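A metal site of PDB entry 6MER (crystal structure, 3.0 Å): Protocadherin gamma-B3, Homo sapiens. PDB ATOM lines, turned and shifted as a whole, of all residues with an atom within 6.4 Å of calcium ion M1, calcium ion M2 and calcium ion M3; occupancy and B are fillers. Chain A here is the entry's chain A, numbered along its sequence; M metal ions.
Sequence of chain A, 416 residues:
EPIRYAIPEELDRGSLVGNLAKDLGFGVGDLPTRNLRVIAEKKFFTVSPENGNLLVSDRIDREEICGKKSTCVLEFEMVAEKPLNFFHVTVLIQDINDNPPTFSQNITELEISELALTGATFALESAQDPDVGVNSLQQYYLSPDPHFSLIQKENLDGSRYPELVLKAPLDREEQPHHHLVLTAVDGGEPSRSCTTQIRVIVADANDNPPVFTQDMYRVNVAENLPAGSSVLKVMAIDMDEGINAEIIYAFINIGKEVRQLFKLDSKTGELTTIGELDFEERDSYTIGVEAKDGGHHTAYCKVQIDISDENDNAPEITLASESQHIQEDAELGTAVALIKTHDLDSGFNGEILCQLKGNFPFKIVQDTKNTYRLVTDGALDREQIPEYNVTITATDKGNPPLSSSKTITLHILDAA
Six residues have an atom within 4 Å of calcium ion M3: Asn 97, Asn 99, Asp 129, Asp 131, Asn 135 and Asp 186.
The nearest printed residue that does not touch calcium ion M3 is Ser 136 (4.7 Å).
Of the 26 residues printed, 6 come within 4 Å of calcium ion M2.
Calcium ion M1 is bound by OD1 of Asp 61 (2.5 Å), OD2 of Asp 98 (2.5 Å), OE1 of Glu 63 (2.6 Å) and OE2 of Glu 10 (2.6 Å).
Slightly farther from calcium ion M1 lies the side-chain carboxylate (OE1) of Glu 9 (3.0 Å).
The nearest printed residue that does not touch calcium ion M1 is Arg 62 (4.2 Å).
The backbone NH of Arg 62 lies within hydrogen-bond range of the side-chain carboxylate of Glu 9, at 2.7 Å.
N of Glu 9 sits at hydrogen-bond distance from O of Gln 94 (3.2 Å).
The backbone carbonyl oxygen of Asn 97 is in hydrogen-bond range of the guanidinium group of Arg 192.
OD2 of Asp 61 sits at hydrogen-bond distance from N of Glu 64 (2.7 Å).
OD2 of Asp 95 is in hydrogen-bond range of ND2 of Asn 135.
The side-chain carboxylate (OE1) of Glu 10 is in salt-bridge range of the guanidinium group (NE) of Arg 59.
N of Glu 10 lies within hydrogen-bond range of O of Ile 60, 2.9 Å away.
OD1 of Asp 186 is in hydrogen-bond range of N of Arg 192, 2.9 Å away.
Calcium ion M2 is bound by OE2 of Glu 9 (2.4 Å), OD2 of Asp 131 (2.4 Å), OE2 of Glu 63 (2.4 Å), OD1 of Asp 95 (2.5 Å), O of Ile 96 (2.6 Å) and OD1 of Asp 98 (2.7 Å).
Calcium ion M3 is bound by OD1 of Asn 97, 2.5 Å away.
O of Asn 135 binds calcium ion M3, 2.5 Å away.
OD1 of Asp 129 is bound to calcium ion M3.
O of Asn 99 binds calcium ion M3, at 2.6 Å.
OD1 of Asp 131 binds calcium ion M3 (2.6 Å).
The side-chain carboxylate (OD2) of Asp 129 binds calcium ion M3 (2.6 Å).
OD2 of Asp 186 is bound to calcium ion M3.
Calcium ion M3 has seven donor atoms within binding distance.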
ATOM      1  N   GLU A   9     -28.503  -8.054 -16.034  1.00  0.00           N
ATOM      2  CA  GLU A   9     -27.214  -7.507 -15.651  1.00  0.00           C
ATOM      3  C   GLU A   9     -26.750  -6.446 -16.644  1.00  0.00           C
ATOM      4  O   GLU A   9     -27.363  -6.226 -17.687  1.00  0.00           O
ATOM      5  CB  GLU A   9     -26.169  -8.620 -15.551  1.00  0.00           C
ATOM      6  CG  GLU A   9     -26.005  -9.417 -16.826  1.00  0.00           C
ATOM      7  CD  GLU A   9     -24.676 -10.147 -16.892  1.00  0.00           C
ATOM      8  OE1 GLU A   9     -23.749  -9.764 -16.149  1.00  0.00           O
ATOM      9  OE2 GLU A   9     -24.568 -11.107 -17.679  1.00  0.00           O
ATOM     10  N   GLU A  10     -25.651  -5.783 -16.296  1.00  0.00           N
ATOM     11  CA  GLU A  10     -25.003  -4.795 -17.152  1.00  0.00           C
ATOM     12  C   GLU A  10     -25.956  -3.646 -17.504  1.00  0.00           C
ATOM     13  O   GLU A  10     -26.064  -3.232 -18.659  1.00  0.00           O
ATOM     14  CB  GLU A  10     -24.435  -5.450 -18.412  1.00  0.00           C
ATOM     15  CG  GLU A  10     -23.502  -6.621 -18.157  1.00  0.00           C
ATOM     16  CD  GLU A  10     -22.161  -6.205 -17.597  1.00  0.00           C
ATOM     17  OE1 GLU A  10     -21.884  -4.989 -17.521  1.00  0.00           O
ATOM     18  OE2 GLU A  10     -21.362  -7.095 -17.230  1.00  0.00           O
ATOM     19  N   ARG A  59     -21.493  -1.072 -11.927  1.00  0.00           N
ATOM     20  CA  ARG A  59     -21.648  -2.092 -12.955  1.00  0.00           C
ATOM     21  C   ARG A  59     -22.020  -3.433 -12.334  1.00  0.00           C
ATOM     22  O   ARG A  59     -21.349  -3.904 -11.402  1.00  0.00           O
ATOM     23  CB  ARG A  59     -20.354  -2.222 -13.764  1.00  0.00           C
ATOM     24  CG  ARG A  59     -20.386  -3.301 -14.835  1.00  0.00           C
ATOM     25  CD  ARG A  59     -19.134  -3.261 -15.693  1.00  0.00           C
ATOM     26  NE  ARG A  59     -19.112  -4.323 -16.689  1.00  0.00           N
ATOM     27  CZ  ARG A  59     -18.456  -5.470 -16.546  1.00  0.00           C
ATOM     28  NH1 ARG A  59     -17.762  -5.714 -15.437  1.00  0.00           N
ATOM     29  NH2 ARG A  59     -18.488  -6.380 -17.513  1.00  0.00           N
ATOM     30  N   ILE A  60     -23.078  -4.041 -12.841  1.00  0.00           N
ATOM     31  CA  ILE A  60     -23.582  -5.315 -12.330  1.00  0.00           C
ATOM     32  C   ILE A  60     -23.126  -6.389 -13.306  1.00  0.00           C
ATOM     33  O   ILE A  60     -23.814  -6.704 -14.287  1.00  0.00           O
ATOM     34  CB  ILE A  60     -25.098  -5.303 -12.145  1.00  0.00           C
ATOM     35  CG1 ILE A  60     -25.526  -4.080 -11.325  1.00  0.00           C
ATOM     36  CG2 ILE A  60     -25.559  -6.577 -11.457  1.00  0.00           C
ATOM     37  CD1 ILE A  60     -24.941  -4.031  -9.933  1.00  0.00           C
ATOM     38  N   ASP A  61     -21.960  -6.965 -13.047  1.00  0.00           N
ATOM     39  CA  ASP A  61     -21.415  -8.048 -13.855  1.00  0.00           C
ATOM     40  C   ASP A  61     -21.741  -9.365 -13.150  1.00  0.00           C
ATOM     41  O   ASP A  61     -21.236  -9.629 -12.056  1.00  0.00           O
ATOM     42  CB  ASP A  61     -19.911  -7.887 -14.056  1.00  0.00           C
ATOM     43  CG  ASP A  61     -19.304  -8.983 -14.909  1.00  0.00           C
ATOM     44  OD1 ASP A  61     -19.511  -8.959 -16.146  1.00  0.00           O
ATOM     45  OD2 ASP A  61     -18.625  -9.868 -14.358  1.00  0.00           O
ATOM     46  N   ARG A  62     -22.572 -10.182 -13.786  1.00  0.00           N
ATOM     47  CA  ARG A  62     -22.994 -11.436 -13.157  1.00  0.00           C
ATOM     48  C   ARG A  62     -21.845 -12.428 -13.052  1.00  0.00           C
ATOM     49  O   ARG A  62     -21.845 -13.293 -12.165  1.00  0.00           O
ATOM     50  CB  ARG A  62     -24.156 -12.054 -13.938  1.00  0.00           C
ATOM     51  CG  ARG A  62     -24.900 -13.137 -13.164  1.00  0.00           C
ATOM     52  CD  ARG A  62     -25.512 -14.157 -14.115  1.00  0.00           C
ATOM     53  NE  ARG A  62     -24.487 -14.866 -14.862  1.00  0.00           N
ATOM     54  CZ  ARG A  62     -23.835 -15.935 -14.417  1.00  0.00           C
ATOM     55  NH1 ARG A  62     -24.109 -16.423 -13.215  1.00  0.00           N
ATOM     56  NH2 ARG A  62     -22.912 -16.517 -15.167  1.00  0.00           N
ATOM     57  N   GLU A  63     -20.850 -12.331 -13.946  1.00  0.00           N
ATOM     58  CA  GLU A  63     -19.719 -13.253 -13.910  1.00  0.00           C
ATOM     59  C   GLU A  63     -18.738 -12.920 -12.792  1.00  0.00           C
ATOM     60  O   GLU A  63     -18.039 -13.817 -12.301  1.00  0.00           O
ATOM     61  CB  GLU A  63     -18.995 -13.252 -15.258  1.00  0.00           C
ATOM     62  CG  GLU A  63     -19.730 -13.998 -16.364  1.00  0.00           C
ATOM     63  CD  GLU A  63     -20.980 -13.274 -16.830  1.00  0.00           C
ATOM     64  OE1 GLU A  63     -20.952 -12.032 -16.933  1.00  0.00           O
ATOM     65  OE2 GLU A  63     -21.994 -13.949 -17.108  1.00  0.00           O
ATOM     66  N   GLU A  64     -18.681 -11.660 -12.377  1.00  0.00           N
ATOM     67  CA  GLU A  64     -17.806 -11.281 -11.266  1.00  0.00           C
ATOM     68  C   GLU A  64     -18.430 -11.612  -9.921  1.00  0.00           C
ATOM     69  O   GLU A  64     -17.711 -11.844  -8.940  1.00  0.00           O
ATOM     70  CB  GLU A  64     -17.484  -9.784 -11.351  1.00  0.00           C
ATOM     71  CG  GLU A  64     -16.521  -9.280 -10.284  1.00  0.00           C
ATOM     72  CD  GLU A  64     -15.105  -9.785 -10.483  1.00  0.00           C
ATOM     73  OE1 GLU A  64     -14.776 -10.214 -11.604  1.00  0.00           O
ATOM     74  OE2 GLU A  64     -14.316  -9.754  -9.506  1.00  0.00           O
ATOM     75  N   GLN A  94     -30.372 -11.431 -13.750  1.00  0.00           N
ATOM     76  CA  GLN A  94     -30.579 -12.296 -14.898  1.00  0.00           C
ATOM     77  C   GLN A  94     -29.360 -12.263 -15.811  1.00  0.00           C
ATOM     78  O   GLN A  94     -28.729 -11.214 -15.986  1.00  0.00           O
ATOM     79  CB  GLN A  94     -31.828 -11.877 -15.665  1.00  0.00           C
ATOM     80  CG  GLN A  94     -33.115 -12.014 -14.858  1.00  0.00           C
ATOM     81  CD  GLN A  94     -34.332 -11.488 -15.606  1.00  0.00           C
ATOM     82  OE1 GLN A  94     -34.208 -10.661 -16.511  1.00  0.00           O
ATOM     83  NE2 GLN A  94     -35.503 -11.972 -15.228  1.00  0.00           N
ATOM     84  N   ASP A  95     -29.030 -13.412 -16.383  1.00  0.00           N
ATOM     85  CA  ASP A  95     -27.849 -13.556 -17.223  1.00  0.00           C
ATOM     86  C   ASP A  95     -28.164 -13.160 -18.657  1.00  0.00           C
ATOM     87  O   ASP A  95     -29.158 -13.622 -19.234  1.00  0.00           O
ATOM     88  CB  ASP A  95     -27.328 -14.987 -17.178  1.00  0.00           C
ATOM     89  CG  ASP A  95     -26.135 -15.214 -18.081  1.00  0.00           C
ATOM     90  OD1 ASP A  95     -25.032 -14.730 -17.752  1.00  0.00           O
ATOM     91  OD2 ASP A  95     -26.296 -15.876 -19.134  1.00  0.00           O
ATOM     92  N   ILE A  96     -27.317 -12.304 -19.231  1.00  0.00           N
ATOM     93  CA  ILE A  96     -27.406 -11.938 -20.646  1.00  0.00           C
ATOM     94  C   ILE A  96     -26.181 -12.510 -21.353  1.00  0.00           C
ATOM     95  O   ILE A  96     -25.112 -12.673 -20.753  1.00  0.00           O
ATOM     96  CB  ILE A  96     -27.498 -10.409 -20.847  1.00  0.00           C
ATOM     97  CG1 ILE A  96     -26.205  -9.724 -20.416  1.00  0.00           C
ATOM     98  CG2 ILE A  96     -28.691  -9.843 -20.097  1.00  0.00           C
ATOM     99  CD1 ILE A  96     -26.194  -8.231 -20.642  1.00  0.00           C
ATOM    100  N   ASN A  97     -26.353 -12.817 -22.636  1.00  0.00           N
ATOM    101  CA  ASN A  97     -25.282 -13.412 -23.433  1.00  0.00           C
ATOM    102  C   ASN A  97     -24.360 -12.303 -23.925  1.00  0.00           C
ATOM    103  O   ASN A  97     -24.404 -11.868 -25.087  1.00  0.00           O
ATOM    104  CB  ASN A  97     -25.866 -14.215 -24.593  1.00  0.00           C
ATOM    105  CG  ASN A  97     -24.806 -14.985 -25.349  1.00  0.00           C
ATOM    106  OD1 ASN A  97     -23.706 -15.234 -24.830  1.00  0.00           O
ATOM    107  ND2 ASN A  97     -25.105 -15.369 -26.583  1.00  0.00           N
ATOM    108  N   ASP A  98     -23.503 -11.832 -23.019  1.00  0.00           N
ATOM    109  CA  ASP A  98     -22.559 -10.768 -23.319  1.00  0.00           C
ATOM    110  C   ASP A  98     -21.123 -11.261 -23.413  1.00  0.00           C
ATOM    111  O   ASP A  98     -20.236 -10.474 -23.749  1.00  0.00           O
ATOM    112  CB  ASP A  98     -22.653  -9.664 -22.265  1.00  0.00           C
ATOM    113  CG  ASP A  98     -22.521 -10.188 -20.842  1.00  0.00           C
ATOM    114  OD1 ASP A  98     -22.427 -11.424 -20.663  1.00  0.00           O
ATOM    115  OD2 ASP A  98     -22.502  -9.364 -19.906  1.00  0.00           O
ATOM    116  N   ASN A  99     -20.876 -12.541 -23.146  1.00  0.00           N
ATOM    117  CA  ASN A  99     -19.541 -13.109 -23.224  1.00  0.00           C
ATOM    118  C   ASN A  99     -19.500 -14.184 -24.301  1.00  0.00           C
ATOM    119  O   ASN A  99     -20.357 -15.081 -24.317  1.00  0.00           O
ATOM    120  CB  ASN A  99     -19.111 -13.704 -21.871  1.00  0.00           C
ATOM    121  CG  ASN A  99     -18.911 -12.639 -20.808  1.00  0.00           C
ATOM    122  OD1 ASN A  99     -19.653 -12.572 -19.830  1.00  0.00           O
ATOM    123  ND2 ASN A  99     -17.895 -11.807 -20.995  1.00  0.00           N
ATOM    124  N   PRO A 100     -18.532 -14.135 -25.213  1.00  0.00           N
ATOM    125  CA  PRO A 100     -18.437 -15.160 -26.252  1.00  0.00           C
ATOM    126  C   PRO A 100     -17.700 -16.386 -25.731  1.00  0.00           C
ATOM    127  O   PRO A 100     -16.954 -16.300 -24.749  1.00  0.00           O
ATOM    128  CB  PRO A 100     -17.651 -14.461 -27.358  1.00  0.00           C
ATOM    129  CG  PRO A 100     -16.747 -13.527 -26.611  1.00  0.00           C
ATOM    130  CD  PRO A 100     -17.524 -13.082 -25.396  1.00  0.00           C
ATOM    131  N   PRO A 101     -17.894 -17.537 -26.378  1.00  0.00           N
ATOM    132  CA  PRO A 101     -17.117 -18.721 -25.996  1.00  0.00           C
ATOM    133  C   PRO A 101     -15.640 -18.529 -26.309  1.00  0.00           C
ATOM    134  O   PRO A 101     -15.246 -17.696 -27.119  1.00  0.00           O
ATOM    135  CB  PRO A 101     -17.720 -19.838 -26.854  1.00  0.00           C
ATOM    136  CG  PRO A 101     -19.057 -19.328 -27.281  1.00  0.00           C
ATOM    137  CD  PRO A 101     -18.893 -17.846 -27.401  1.00  0.00           C
ATOM    138  N   ASP A 129     -17.641 -20.986 -21.482  1.00  0.00           N
ATOM    139  CA  ASP A 129     -18.493 -19.807 -21.601  1.00  0.00           C
ATOM    140  C   ASP A 129     -18.759 -19.276 -20.193  1.00  0.00           C
ATOM    141  O   ASP A 129     -19.307 -20.020 -19.356  1.00  0.00           O
ATOM    142  CB  ASP A 129     -19.806 -20.142 -22.319  1.00  0.00           C
ATOM    143  CG  ASP A 129     -20.346 -18.971 -23.114  1.00  0.00           C
ATOM    144  OD1 ASP A 129     -20.015 -17.818 -22.784  1.00  0.00           O
ATOM    145  OD2 ASP A 129     -21.106 -19.211 -24.075  1.00  0.00           O
ATOM    146  N   PRO A 130     -18.390 -18.035 -19.888  1.00  0.00           N
ATOM    147  CA  PRO A 130     -18.601 -17.521 -18.529  1.00  0.00           C
ATOM    148  C   PRO A 130     -20.065 -17.390 -18.133  1.00  0.00           C
ATOM    149  O   PRO A 130     -20.360 -17.303 -16.932  1.00  0.00           O
ATOM    150  CB  PRO A 130     -17.914 -16.149 -18.552  1.00  0.00           C
ATOM    151  CG  PRO A 130     -16.974 -16.205 -19.717  1.00  0.00           C
ATOM    152  CD  PRO A 130     -17.649 -17.077 -20.728  1.00  0.00           C
ATOM    153  N   ASP A 131     -20.979 -17.383 -19.093  1.00  0.00           N
ATOM    154  CA  ASP A 131     -22.402 -17.232 -18.787  1.00  0.00           C
ATOM    155  C   ASP A 131     -22.979 -18.556 -18.298  1.00  0.00           C
ATOM    156  O   ASP A 131     -22.284 -19.569 -18.183  1.00  0.00           O
ATOM    157  CB  ASP A 131     -23.154 -16.725 -20.020  1.00  0.00           C
ATOM    158  CG  ASP A 131     -22.435 -15.576 -20.704  1.00  0.00           C
ATOM    159  OD1 ASP A 131     -21.473 -15.844 -21.448  1.00  0.00           O
ATOM    160  OD2 ASP A 131     -22.837 -14.420 -20.499  1.00  0.00           O
ATOM    161  N   VAL A 132     -24.276 -18.553 -17.996  1.00  0.00           N
ATOM    162  CA  VAL A 132     -24.995 -19.737 -17.543  1.00  0.00           C
ATOM    163  C   VAL A 132     -26.261 -19.890 -18.363  1.00  0.00           C
ATOM    164  O   VAL A 132     -26.635 -19.017 -19.154  1.00  0.00           O
ATOM    165  CB  VAL A 132     -25.324 -19.678 -16.037  1.00  0.00           C
ATOM    166  CG1 VAL A 132     -24.060 -19.672 -15.201  1.00  0.00           C
ATOM    167  CG2 VAL A 132     -26.172 -18.450 -15.727  1.00  0.00           C
ATOM    168  N   VAL A 134     -28.930 -21.061 -21.149  1.00  0.00           N
ATOM    169  CA  VAL A 134     -28.840 -21.221 -22.595  1.00  0.00           C
ATOM    170  C   VAL A 134     -27.705 -20.397 -23.182  1.00  0.00           C
ATOM    171  O   VAL A 134     -27.220 -20.711 -24.272  1.00  0.00           O
ATOM    172  CB  VAL A 134     -30.180 -20.872 -23.266  1.00  0.00           C
ATOM    173  CG1 VAL A 134     -31.292 -21.775 -22.749  1.00  0.00           C
ATOM    174  CG2 VAL A 134     -30.527 -19.406 -23.030  1.00  0.00           C
ATOM    175  N   ASN A 135     -27.260 -19.351 -22.488  1.00  0.00           N
ATOM    176  CA  ASN A 135     -26.143 -18.547 -22.956  1.00  0.00           C
ATOM    177  C   ASN A 135     -24.809 -19.262 -22.803  1.00  0.00           C
ATOM    178  O   ASN A 135     -23.785 -18.719 -23.243  1.00  0.00           O
ATOM    179  CB  ASN A 135     -26.107 -17.219 -22.215  1.00  0.00           C
ATOM    180  CG  ASN A 135     -27.407 -16.452 -22.315  1.00  0.00           C
ATOM    181  OD1 ASN A 135     -28.085 -16.492 -23.341  1.00  0.00           O
ATOM    182  ND2 ASN A 135     -27.779 -15.763 -21.238  1.00  0.00           N
ATOM    183  N   SER A 136     -24.788 -20.444 -22.190  1.00  0.00           N
ATOM    184  CA  SER A 136     -23.574 -21.232 -22.037  1.00  0.00           C
ATOM    185  C   SER A 136     -23.589 -22.538 -22.821  1.00  0.00           C
ATOM    186  O   SER A 136     -22.521 -23.088 -23.085  1.00  0.00           O
ATOM    187  CB  SER A 136     -23.310 -21.541 -20.562  1.00  0.00           C
ATOM    188  OG  SER A 136     -22.105 -22.256 -20.390  1.00  0.00           O
ATOM    189  N   GLN A 138     -23.334 -24.815 -25.798  1.00  0.00           N
ATOM    190  CA  GLN A 138     -22.591 -24.602 -27.026  1.00  0.00           C
ATOM    191  C   GLN A 138     -23.026 -25.564 -28.120  1.00  0.00           C
ATOM    192  O   GLN A 138     -23.435 -26.700 -27.851  1.00  0.00           O
ATOM    193  CB  GLN A 138     -21.077 -24.761 -26.787  1.00  0.00           C
ATOM    194  CG  GLN A 138     -20.519 -23.803 -25.748  1.00  0.00           C
ATOM    195  CD  GLN A 138     -20.641 -22.357 -26.167  1.00  0.00           C
ATOM    196  OE1 GLN A 138     -20.718 -22.040 -27.361  1.00  0.00           O
ATOM    197  NE2 GLN A 138     -20.656 -21.460 -25.187  1.00  0.00           N
ATOM    198  N   ASP A 186     -22.747 -20.384 -29.005  1.00  0.00           N
ATOM    199  CA  ASP A 186     -23.671 -20.545 -27.894  1.00  0.00           C
ATOM    200  C   ASP A 186     -25.099 -20.263 -28.339  1.00  0.00           C
ATOM    201  O   ASP A 186     -25.355 -19.723 -29.416  1.00  0.00           O
ATOM    202  CB  ASP A 186     -23.272 -19.647 -26.728  1.00  0.00           C
ATOM    203  CG  ASP A 186     -23.093 -18.191 -27.127  1.00  0.00           C
ATOM    204  OD1 ASP A 186     -23.439 -17.834 -28.278  1.00  0.00           O
ATOM    205  OD2 ASP A 186     -22.613 -17.398 -26.294  1.00  0.00           O
ATOM    206  N   ARG A 192     -23.048 -15.528 -29.976  1.00  0.00           N
ATOM    207  CA  ARG A 192     -21.624 -15.250 -30.077  1.00  0.00           C
ATOM    208  C   ARG A 192     -20.858 -16.521 -30.423  1.00  0.00           C
ATOM    209  O   ARG A 192     -21.228 -17.625 -30.007  1.00  0.00           O
ATOM    210  CB  ARG A 192     -21.101 -14.659 -28.772  1.00  0.00           C
ATOM    211  CG  ARG A 192     -21.836 -13.394 -28.352  1.00  0.00           C
ATOM    212  CD  ARG A 192     -21.201 -12.744 -27.126  1.00  0.00           C
ATOM    213  NE  ARG A 192     -21.892 -11.524 -26.752  1.00  0.00           N
ATOM    214  CZ  ARG A 192     -21.625 -10.328 -27.263  1.00  0.00           C
ATOM    215  NH1 ARG A 192     -20.679 -10.189 -28.177  1.00  0.00           N
ATOM    216  NH2 ARG A 192     -22.306  -9.261 -26.870  1.00  0.00           N
HETATM  217 CA    CA M   1     -21.266  -9.617 -17.762  1.00  0.00          CA
HETATM  218 CA    CA M   2     -23.512 -12.962 -18.737  1.00  0.00          CA
HETATM  219 CA    CA M   3     -22.179 -16.838 -23.758  1.00  0.00          CA
